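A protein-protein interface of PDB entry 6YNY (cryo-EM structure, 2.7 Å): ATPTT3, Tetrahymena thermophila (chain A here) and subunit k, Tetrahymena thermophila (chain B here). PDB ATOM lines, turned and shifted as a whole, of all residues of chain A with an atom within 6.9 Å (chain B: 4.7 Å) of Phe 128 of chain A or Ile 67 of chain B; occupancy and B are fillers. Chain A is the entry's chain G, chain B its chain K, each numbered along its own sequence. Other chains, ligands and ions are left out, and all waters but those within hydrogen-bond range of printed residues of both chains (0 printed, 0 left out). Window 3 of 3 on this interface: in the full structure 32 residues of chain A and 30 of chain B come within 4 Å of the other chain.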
ATOM      1  N   SER A 115      -7.805  19.475  -5.068  1.00  0.00           N
ATOM      2  CA  SER A 115      -8.508  20.723  -5.332  1.00  0.00           C
ATOM      3  C   SER A 115      -9.272  21.206  -4.109  1.00  0.00           C
ATOM      4  O   SER A 115      -9.432  22.416  -3.918  1.00  0.00           O
ATOM      5  CB  SER A 115      -9.461  20.544  -6.511  1.00  0.00           C
ATOM      6  OG  SER A 115     -10.142  21.748  -6.805  1.00  0.00           O
ATOM      7  N   PHE A 117      -8.386  20.523  -0.848  1.00  0.00           N
ATOM      8  CA  PHE A 117      -7.477  20.896   0.227  1.00  0.00           C
ATOM      9  C   PHE A 117      -7.106  22.369   0.145  1.00  0.00           C
ATOM     10  O   PHE A 117      -7.017  23.053   1.171  1.00  0.00           O
ATOM     11  CB  PHE A 117      -6.228  20.023   0.176  1.00  0.00           C
ATOM     12  CG  PHE A 117      -5.251  20.302   1.276  1.00  0.00           C
ATOM     13  CD1 PHE A 117      -5.452  19.787   2.541  1.00  0.00           C
ATOM     14  CD2 PHE A 117      -4.132  21.078   1.045  1.00  0.00           C
ATOM     15  CE1 PHE A 117      -4.556  20.042   3.556  1.00  0.00           C
ATOM     16  CE2 PHE A 117      -3.233  21.336   2.056  1.00  0.00           C
ATOM     17  CZ  PHE A 117      -3.444  20.816   3.313  1.00  0.00           C
ATOM     18  N   PHE A 118      -6.887  22.877  -1.065  1.00  0.00           N
ATOM     19  CA  PHE A 118      -6.541  24.278  -1.251  1.00  0.00           C
ATOM     20  C   PHE A 118      -7.757  25.183  -1.368  1.00  0.00           C
ATOM     21  O   PHE A 118      -7.628  26.396  -1.177  1.00  0.00           O
ATOM     22  CB  PHE A 118      -5.674  24.445  -2.498  1.00  0.00           C
ATOM     23  CG  PHE A 118      -4.364  23.724  -2.424  1.00  0.00           C
ATOM     24  CD1 PHE A 118      -3.341  24.196  -1.628  1.00  0.00           C
ATOM     25  CD2 PHE A 118      -4.154  22.576  -3.159  1.00  0.00           C
ATOM     26  CE1 PHE A 118      -2.139  23.533  -1.562  1.00  0.00           C
ATOM     27  CE2 PHE A 118      -2.953  21.911  -3.097  1.00  0.00           C
ATOM     28  CZ  PHE A 118      -1.945  22.390  -2.298  1.00  0.00           C
ATOM     29  N   TYR A 119      -8.932  24.628  -1.673  1.00  0.00           N
ATOM     30  CA  TYR A 119     -10.130  25.452  -1.755  1.00  0.00           C
ATOM     31  C   TYR A 119     -10.536  25.985  -0.390  1.00  0.00           C
ATOM     32  O   TYR A 119     -11.182  27.034  -0.302  1.00  0.00           O
ATOM     33  CB  TYR A 119     -11.274  24.652  -2.369  1.00  0.00           C
ATOM     34  CG  TYR A 119     -12.556  25.435  -2.518  1.00  0.00           C
ATOM     35  CD1 TYR A 119     -12.706  26.370  -3.527  1.00  0.00           C
ATOM     36  CD2 TYR A 119     -13.616  25.235  -1.651  1.00  0.00           C
ATOM     37  CE1 TYR A 119     -13.874  27.088  -3.667  1.00  0.00           C
ATOM     38  CE2 TYR A 119     -14.789  25.946  -1.782  1.00  0.00           C
ATOM     39  CZ  TYR A 119     -14.912  26.871  -2.793  1.00  0.00           C
ATOM     40  OH  TYR A 119     -16.080  27.584  -2.927  1.00  0.00           O
ATOM     41  N   GLN A 120     -10.170  25.281   0.681  1.00  0.00           N
ATOM     42  CA  GLN A 120     -10.470  25.764   2.020  1.00  0.00           C
ATOM     43  C   GLN A 120      -9.645  26.988   2.384  1.00  0.00           C
ATOM     44  O   GLN A 120      -9.995  27.695   3.334  1.00  0.00           O
ATOM     45  CB  GLN A 120     -10.229  24.654   3.040  1.00  0.00           C
ATOM     46  CG  GLN A 120     -10.937  23.360   2.714  1.00  0.00           C
ATOM     47  CD  GLN A 120     -12.435  23.531   2.595  1.00  0.00           C
ATOM     48  OE1 GLN A 120     -13.014  24.458   3.159  1.00  0.00           O
ATOM     49  NE2 GLN A 120     -13.072  22.638   1.850  1.00  0.00           N
ATOM     50  N   PHE A 121      -8.564  27.251   1.651  1.00  0.00           N
ATOM     51  CA  PHE A 121      -7.694  28.390   1.914  1.00  0.00           C
ATOM     52  C   PHE A 121      -7.701  29.387   0.761  1.00  0.00           C
ATOM     53  O   PHE A 121      -6.824  30.253   0.690  1.00  0.00           O
ATOM     54  CB  PHE A 121      -6.270  27.910   2.184  1.00  0.00           C
ATOM     55  CG  PHE A 121      -6.185  26.806   3.192  1.00  0.00           C
ATOM     56  CD1 PHE A 121      -5.953  25.506   2.791  1.00  0.00           C
ATOM     57  CD2 PHE A 121      -6.339  27.067   4.540  1.00  0.00           C
ATOM     58  CE1 PHE A 121      -5.872  24.487   3.714  1.00  0.00           C
ATOM     59  CE2 PHE A 121      -6.259  26.049   5.467  1.00  0.00           C
ATOM     60  CZ  PHE A 121      -6.027  24.757   5.052  1.00  0.00           C
ATOM     61  N   ALA A 122      -8.677  29.285  -0.142  1.00  0.00           N
ATOM     62  CA  ALA A 122      -8.703  30.169  -1.302  1.00  0.00           C
ATOM     63  C   ALA A 122      -8.881  31.625  -0.900  1.00  0.00           C
ATOM     64  O   ALA A 122      -8.468  32.527  -1.638  1.00  0.00           O
ATOM     65  CB  ALA A 122      -9.818  29.745  -2.253  1.00  0.00           C
ATOM     66  N   ASP A 123      -9.488  31.878   0.258  1.00  0.00           N
ATOM     67  CA  ASP A 123      -9.699  33.242   0.724  1.00  0.00           C
ATOM     68  C   ASP A 123      -8.465  33.843   1.379  1.00  0.00           C
ATOM     69  O   ASP A 123      -8.423  35.062   1.578  1.00  0.00           O
ATOM     70  CB  ASP A 123     -10.865  33.278   1.712  1.00  0.00           C
ATOM     71  CG  ASP A 123     -10.639  32.381   2.910  1.00  0.00           C
ATOM     72  OD1 ASP A 123      -9.948  31.353   2.758  1.00  0.00           O
ATOM     73  OD2 ASP A 123     -11.154  32.700   4.002  1.00  0.00           O
ATOM     74  N   LEU A 124      -7.466  33.029   1.713  1.00  0.00           N
ATOM     75  CA  LEU A 124      -6.268  33.553   2.359  1.00  0.00           C
ATOM     76  C   LEU A 124      -5.365  34.270   1.367  1.00  0.00           C
ATOM     77  O   LEU A 124      -4.783  35.311   1.695  1.00  0.00           O
ATOM     78  CB  LEU A 124      -5.506  32.418   3.040  1.00  0.00           C
ATOM     79  CG  LEU A 124      -6.032  31.964   4.399  1.00  0.00           C
ATOM     80  CD1 LEU A 124      -7.498  31.600   4.318  1.00  0.00           C
ATOM     81  CD2 LEU A 124      -5.220  30.787   4.900  1.00  0.00           C
ATOM     82  N   ALA A 125      -5.234  33.735   0.158  1.00  0.00           N
ATOM     83  CA  ALA A 125      -4.371  34.338  -0.846  1.00  0.00           C
ATOM     84  C   ALA A 125      -4.733  33.770  -2.209  1.00  0.00           C
ATOM     85  O   ALA A 125      -5.533  32.840  -2.328  1.00  0.00           O
ATOM     86  CB  ALA A 125      -2.896  34.094  -0.527  1.00  0.00           C
ATOM     87  N   LEU A 126      -4.122  34.347  -3.243  1.00  0.00           N
ATOM     88  CA  LEU A 126      -4.379  33.906  -4.607  1.00  0.00           C
ATOM     89  C   LEU A 126      -3.686  32.588  -4.917  1.00  0.00           C
ATOM     90  O   LEU A 126      -4.141  31.845  -5.793  1.00  0.00           O
ATOM     91  CB  LEU A 126      -3.918  34.979  -5.593  1.00  0.00           C
ATOM     92  CG  LEU A 126      -4.074  34.679  -7.085  1.00  0.00           C
ATOM     93  CD1 LEU A 126      -5.534  34.605  -7.483  1.00  0.00           C
ATOM     94  CD2 LEU A 126      -3.351  35.730  -7.898  1.00  0.00           C
ATOM     95  N   GLY A 127      -2.593  32.283  -4.219  1.00  0.00           N
ATOM     96  CA  GLY A 127      -1.851  31.075  -4.523  1.00  0.00           C
ATOM     97  C   GLY A 127      -2.657  29.811  -4.313  1.00  0.00           C
ATOM     98  O   GLY A 127      -2.409  28.797  -4.968  1.00  0.00           O
ATOM     99  N   PHE A 128      -3.630  29.850  -3.405  1.00  0.00           N
ATOM    100  CA  PHE A 128      -4.461  28.677  -3.171  1.00  0.00           C
ATOM    101  C   PHE A 128      -5.505  28.497  -4.261  1.00  0.00           C
ATOM    102  O   PHE A 128      -5.868  27.361  -4.584  1.00  0.00           O
ATOM    103  CB  PHE A 128      -5.142  28.778  -1.811  1.00  0.00           C
ATOM    104  CG  PHE A 128      -4.188  28.826  -0.658  1.00  0.00           C
ATOM    105  CD1 PHE A 128      -3.597  27.672  -0.184  1.00  0.00           C
ATOM    106  CD2 PHE A 128      -3.884  30.025  -0.046  1.00  0.00           C
ATOM    107  CE1 PHE A 128      -2.722  27.714   0.875  1.00  0.00           C
ATOM    108  CE2 PHE A 128      -3.010  30.072   1.015  1.00  0.00           C
ATOM    109  CZ  PHE A 128      -2.428  28.915   1.475  1.00  0.00           C
ATOM    110  N   LYS A 129      -6.001  29.594  -4.832  1.00  0.00           N
ATOM    111  CA  LYS A 129      -6.947  29.482  -5.935  1.00  0.00           C
ATOM    112  C   LYS A 129      -6.308  28.790  -7.130  1.00  0.00           C
ATOM    113  O   LYS A 129      -6.962  28.008  -7.829  1.00  0.00           O
ATOM    114  CB  LYS A 129      -7.452  30.864  -6.335  1.00  0.00           C
ATOM    115  CG  LYS A 129      -8.195  31.597  -5.240  1.00  0.00           C
ATOM    116  CD  LYS A 129      -8.709  32.938  -5.727  1.00  0.00           C
ATOM    117  CE  LYS A 129      -9.493  33.659  -4.652  1.00  0.00           C
ATOM    118  NZ  LYS A 129      -8.652  33.991  -3.474  1.00  0.00           N
ATOM    119  N   ILE A 130      -5.029  29.064  -7.375  1.00  0.00           N
ATOM    120  CA  ILE A 130      -4.347  28.465  -8.514  1.00  0.00           C
ATOM    121  C   ILE A 130      -4.129  26.977  -8.277  1.00  0.00           C
ATOM    122  O   ILE A 130      -4.447  26.141  -9.129  1.00  0.00           O
ATOM    123  CB  ILE A 130      -3.021  29.195  -8.782  1.00  0.00           C
ATOM    124  CG1 ILE A 130      -3.295  30.654  -9.144  1.00  0.00           C
ATOM    125  CG2 ILE A 130      -2.250  28.501  -9.881  1.00  0.00           C
ATOM    126  CD1 ILE A 130      -2.055  31.493  -9.300  1.00  0.00           C
ATOM    127  N   MET A 131      -3.584  26.625  -7.113  1.00  0.00           N
ATOM    128  CA  MET A 131      -3.335  25.227  -6.796  1.00  0.00           C
ATOM    129  C   MET A 131      -4.618  24.431  -6.618  1.00  0.00           C
ATOM    130  O   MET A 131      -4.562  23.198  -6.593  1.00  0.00           O
ATOM    131  CB  MET A 131      -2.482  25.127  -5.537  1.00  0.00           C
ATOM    132  CG  MET A 131      -1.161  25.862  -5.634  1.00  0.00           C
ATOM    133  SD  MET A 131      -0.129  25.313  -7.003  1.00  0.00           S
ATOM    134  CE  MET A 131       0.070  23.585  -6.596  1.00  0.00           C
ATOM    135  N   ALA A 132      -5.761  25.100  -6.495  1.00  0.00           N
ATOM    136  CA  ALA A 132      -7.043  24.422  -6.412  1.00  0.00           C
ATOM    137  C   ALA A 132      -7.702  24.248  -7.770  1.00  0.00           C
ATOM    138  O   ALA A 132      -8.544  23.356  -7.925  1.00  0.00           O
ATOM    139  CB  ALA A 132      -7.990  25.194  -5.494  1.00  0.00           C
ATOM    140  N   ALA A 133      -7.341  25.074  -8.749  1.00  0.00           N
ATOM    141  CA  ALA A 133      -7.889  24.973 -10.091  1.00  0.00           C
ATOM    142  C   ALA A 133      -6.991  24.203 -11.044  1.00  0.00           C
ATOM    143  O   ALA A 133      -7.491  23.646 -12.026  1.00  0.00           O
ATOM    144  CB  ALA A 133      -8.139  26.370 -10.664  1.00  0.00           C
ATOM    145  N   GLY B  63       1.604  29.936  -7.584  1.00  0.00           N
ATOM    146  CA  GLY B  63       0.867  29.392  -6.459  1.00  0.00           C
ATOM    147  C   GLY B  63       1.742  29.185  -5.239  1.00  0.00           C
ATOM    148  O   GLY B  63       1.347  29.513  -4.118  1.00  0.00           O
ATOM    149  N   CYS B  64       2.944  28.646  -5.439  1.00  0.00           N
ATOM    150  CA  CYS B  64       3.830  28.388  -4.310  1.00  0.00           C
ATOM    151  C   CYS B  64       4.436  29.676  -3.771  1.00  0.00           C
ATOM    152  O   CYS B  64       4.506  29.870  -2.552  1.00  0.00           O
ATOM    153  CB  CYS B  64       4.923  27.406  -4.722  1.00  0.00           C
ATOM    154  SG  CYS B  64       4.312  25.751  -5.102  1.00  0.00           S
ATOM    155  N   PHE B  65       4.875  30.572  -4.656  1.00  0.00           N
ATOM    156  CA  PHE B  65       5.462  31.825  -4.194  1.00  0.00           C
ATOM    157  C   PHE B  65       4.442  32.658  -3.431  1.00  0.00           C
ATOM    158  O   PHE B  65       4.771  33.278  -2.413  1.00  0.00           O
ATOM    159  CB  PHE B  65       6.019  32.619  -5.374  1.00  0.00           C
ATOM    160  CG  PHE B  65       7.104  31.909  -6.133  1.00  0.00           C
ATOM    161  CD1 PHE B  65       7.804  30.858  -5.566  1.00  0.00           C
ATOM    162  CD2 PHE B  65       7.428  32.302  -7.419  1.00  0.00           C
ATOM    163  CE1 PHE B  65       8.800  30.212  -6.268  1.00  0.00           C
ATOM    164  CE2 PHE B  65       8.423  31.659  -8.123  1.00  0.00           C
ATOM    165  CZ  PHE B  65       9.109  30.614  -7.546  1.00  0.00           C
ATOM    166  N   SER B  66       3.196  32.684  -3.905  1.00  0.00           N
ATOM    167  CA  SER B  66       2.157  33.421  -3.203  1.00  0.00           C
ATOM    168  C   SER B  66       1.783  32.759  -1.887  1.00  0.00           C
ATOM    169  O   SER B  66       1.287  33.439  -0.983  1.00  0.00           O
ATOM    170  CB  SER B  66       0.918  33.548  -4.083  1.00  0.00           C
ATOM    171  OG  SER B  66      -0.106  34.265  -3.420  1.00  0.00           O
ATOM    172  N   ILE B  67       2.007  31.454  -1.763  1.00  0.00           N
ATOM    173  CA  ILE B  67       1.682  30.754  -0.528  1.00  0.00           C
ATOM    174  C   ILE B  67       2.760  30.985   0.521  1.00  0.00           C
ATOM    175  O   ILE B  67       2.468  31.392   1.651  1.00  0.00           O
ATOM    176  CB  ILE B  67       1.476  29.255  -0.812  1.00  0.00           C
ATOM    177  CG1 ILE B  67       0.125  29.031  -1.490  1.00  0.00           C
ATOM    178  CG2 ILE B  67       1.563  28.454   0.466  1.00  0.00           C
ATOM    179  CD1 ILE B  67      -0.034  27.670  -2.122  1.00  0.00           C
ATOM    180  N   ILE B  68       4.024  30.739   0.167  1.00  0.00           N
ATOM    181  CA  ILE B  68       5.104  30.934   1.129  1.00  0.00           C
ATOM    182  C   ILE B  68       5.185  32.392   1.551  1.00  0.00           C
ATOM    183  O   ILE B  68       5.538  32.696   2.698  1.00  0.00           O
ATOM    184  CB  ILE B  68       6.440  30.442   0.546  1.00  0.00           C
ATOM    185  CG1 ILE B  68       6.850  31.294  -0.652  1.00  0.00           C
ATOM    186  CG2 ILE B  68       6.326  28.989   0.139  1.00  0.00           C
ATOM    187  CD1 ILE B  68       8.138  30.841  -1.311  1.00  0.00           C
ATOM    188  N   ASN B  69       4.862  33.315   0.646  1.00  0.00           N
ATOM    189  CA  ASN B  69       4.826  34.723   1.019  1.00  0.00           C
ATOM    190  C   ASN B  69       3.707  34.999   2.011  1.00  0.00           C
ATOM    191  O   ASN B  69       3.836  35.886   2.862  1.00  0.00           O
ATOM    192  CB  ASN B  69       4.657  35.591  -0.224  1.00  0.00           C
ATOM    193  CG  ASN B  69       4.620  37.067   0.099  1.00  0.00           C
ATOM    194  OD1 ASN B  69       5.658  37.718   0.208  1.00  0.00           O
ATOM    195  ND2 ASN B  69       3.419  37.606   0.252  1.00  0.00           N
ATOM    196  N   TYR B  70       2.607  34.254   1.917  1.00  0.00           N
ATOM    197  CA  TYR B  70       1.540  34.374   2.904  1.00  0.00           C
ATOM    198  C   TYR B  70       1.977  33.798   4.244  1.00  0.00           C
ATOM    199  O   TYR B  70       1.786  34.424   5.293  1.00  0.00           O
ATOM    200  CB  TYR B  70       0.286  33.665   2.400  1.00  0.00           C
ATOM    201  CG  TYR B  70      -0.825  33.593   3.416  1.00  0.00           C
ATOM    202  CD1 TYR B  70      -1.778  34.596   3.502  1.00  0.00           C
ATOM    203  CD2 TYR B  70      -0.923  32.521   4.290  1.00  0.00           C
ATOM    204  CE1 TYR B  70      -2.794  34.534   4.428  1.00  0.00           C
ATOM    205  CE2 TYR B  70      -1.934  32.451   5.220  1.00  0.00           C
ATOM    206  CZ  TYR B  70      -2.868  33.460   5.285  1.00  0.00           C
ATOM    207  OH  TYR B  70      -3.881  33.391   6.212  1.00  0.00           O
ATOM    208  N   LEU B  71       2.562  32.601   4.226  1.00  0.00           N
ATOM    209  CA  LEU B  71       3.026  31.987   5.465  1.00  0.00           C
ATOM    210  C   LEU B  71       4.077  32.850   6.147  1.00  0.00           C
ATOM    211  O   LEU B  71       4.131  32.917   7.381  1.00  0.00           O
ATOM    212  CB  LEU B  71       3.583  30.595   5.178  1.00  0.00           C
ATOM    213  CG  LEU B  71       2.618  29.646   4.471  1.00  0.00           C
ATOM    214  CD1 LEU B  71       3.264  28.295   4.239  1.00  0.00           C
ATOM    215  CD2 LEU B  71       1.339  29.501   5.264  1.00  0.00           C
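The backbone NH of Gly 127 of chain A lies within hydrogen-bond range of the side-chain hydroxyl of Ser 66 of chain B.
Among the printed residues, merely in contact across the chains: Leu 124 of chain A with Tyr 70 of chain B (3.2 Å), Gly 127 of chain A with Gly 63 of chain B (3.6 Å), Gly 127 of chain A with Ile 67 of chain B (3.9 Å) and Phe 128 of chain A with Ile 67 of chain B (3.9 Å).
Printed residues of chain B within 4 Å of Gly 127 of chain A: Gly 63 (3.6 Å), Ser 66 (3.3 Å) and Ile 67 (3.9 Å).
Of chain B, only Ile 67 (3.9 Å) comes within 4 Å of Phe 128 of chain A.
Of the printed residues of chain A, Gly 63 of chain B touches Gly 127.
Ile 67 of chain B touches just these residues of chain A: Gly 127 (3.9 Å) and Phe 128 (3.9 Å).
Printed residues of chain A within 4 Å of Tyr 70 of chain B: Leu 124 (3.2 Å).
The nearest residue of chain A that does not touch Ile 67 of chain B is Met 131 of chain A (4.1 Å).
Hydrophobic or aromatic side chains of chain B that line the printed part of chain A: Ile 67 and Tyr 70.
Of the 18 printed residues of chain A, 3 touch a printed residue of chain B.
Among the printed residues, 5 pairs touch across the chains.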
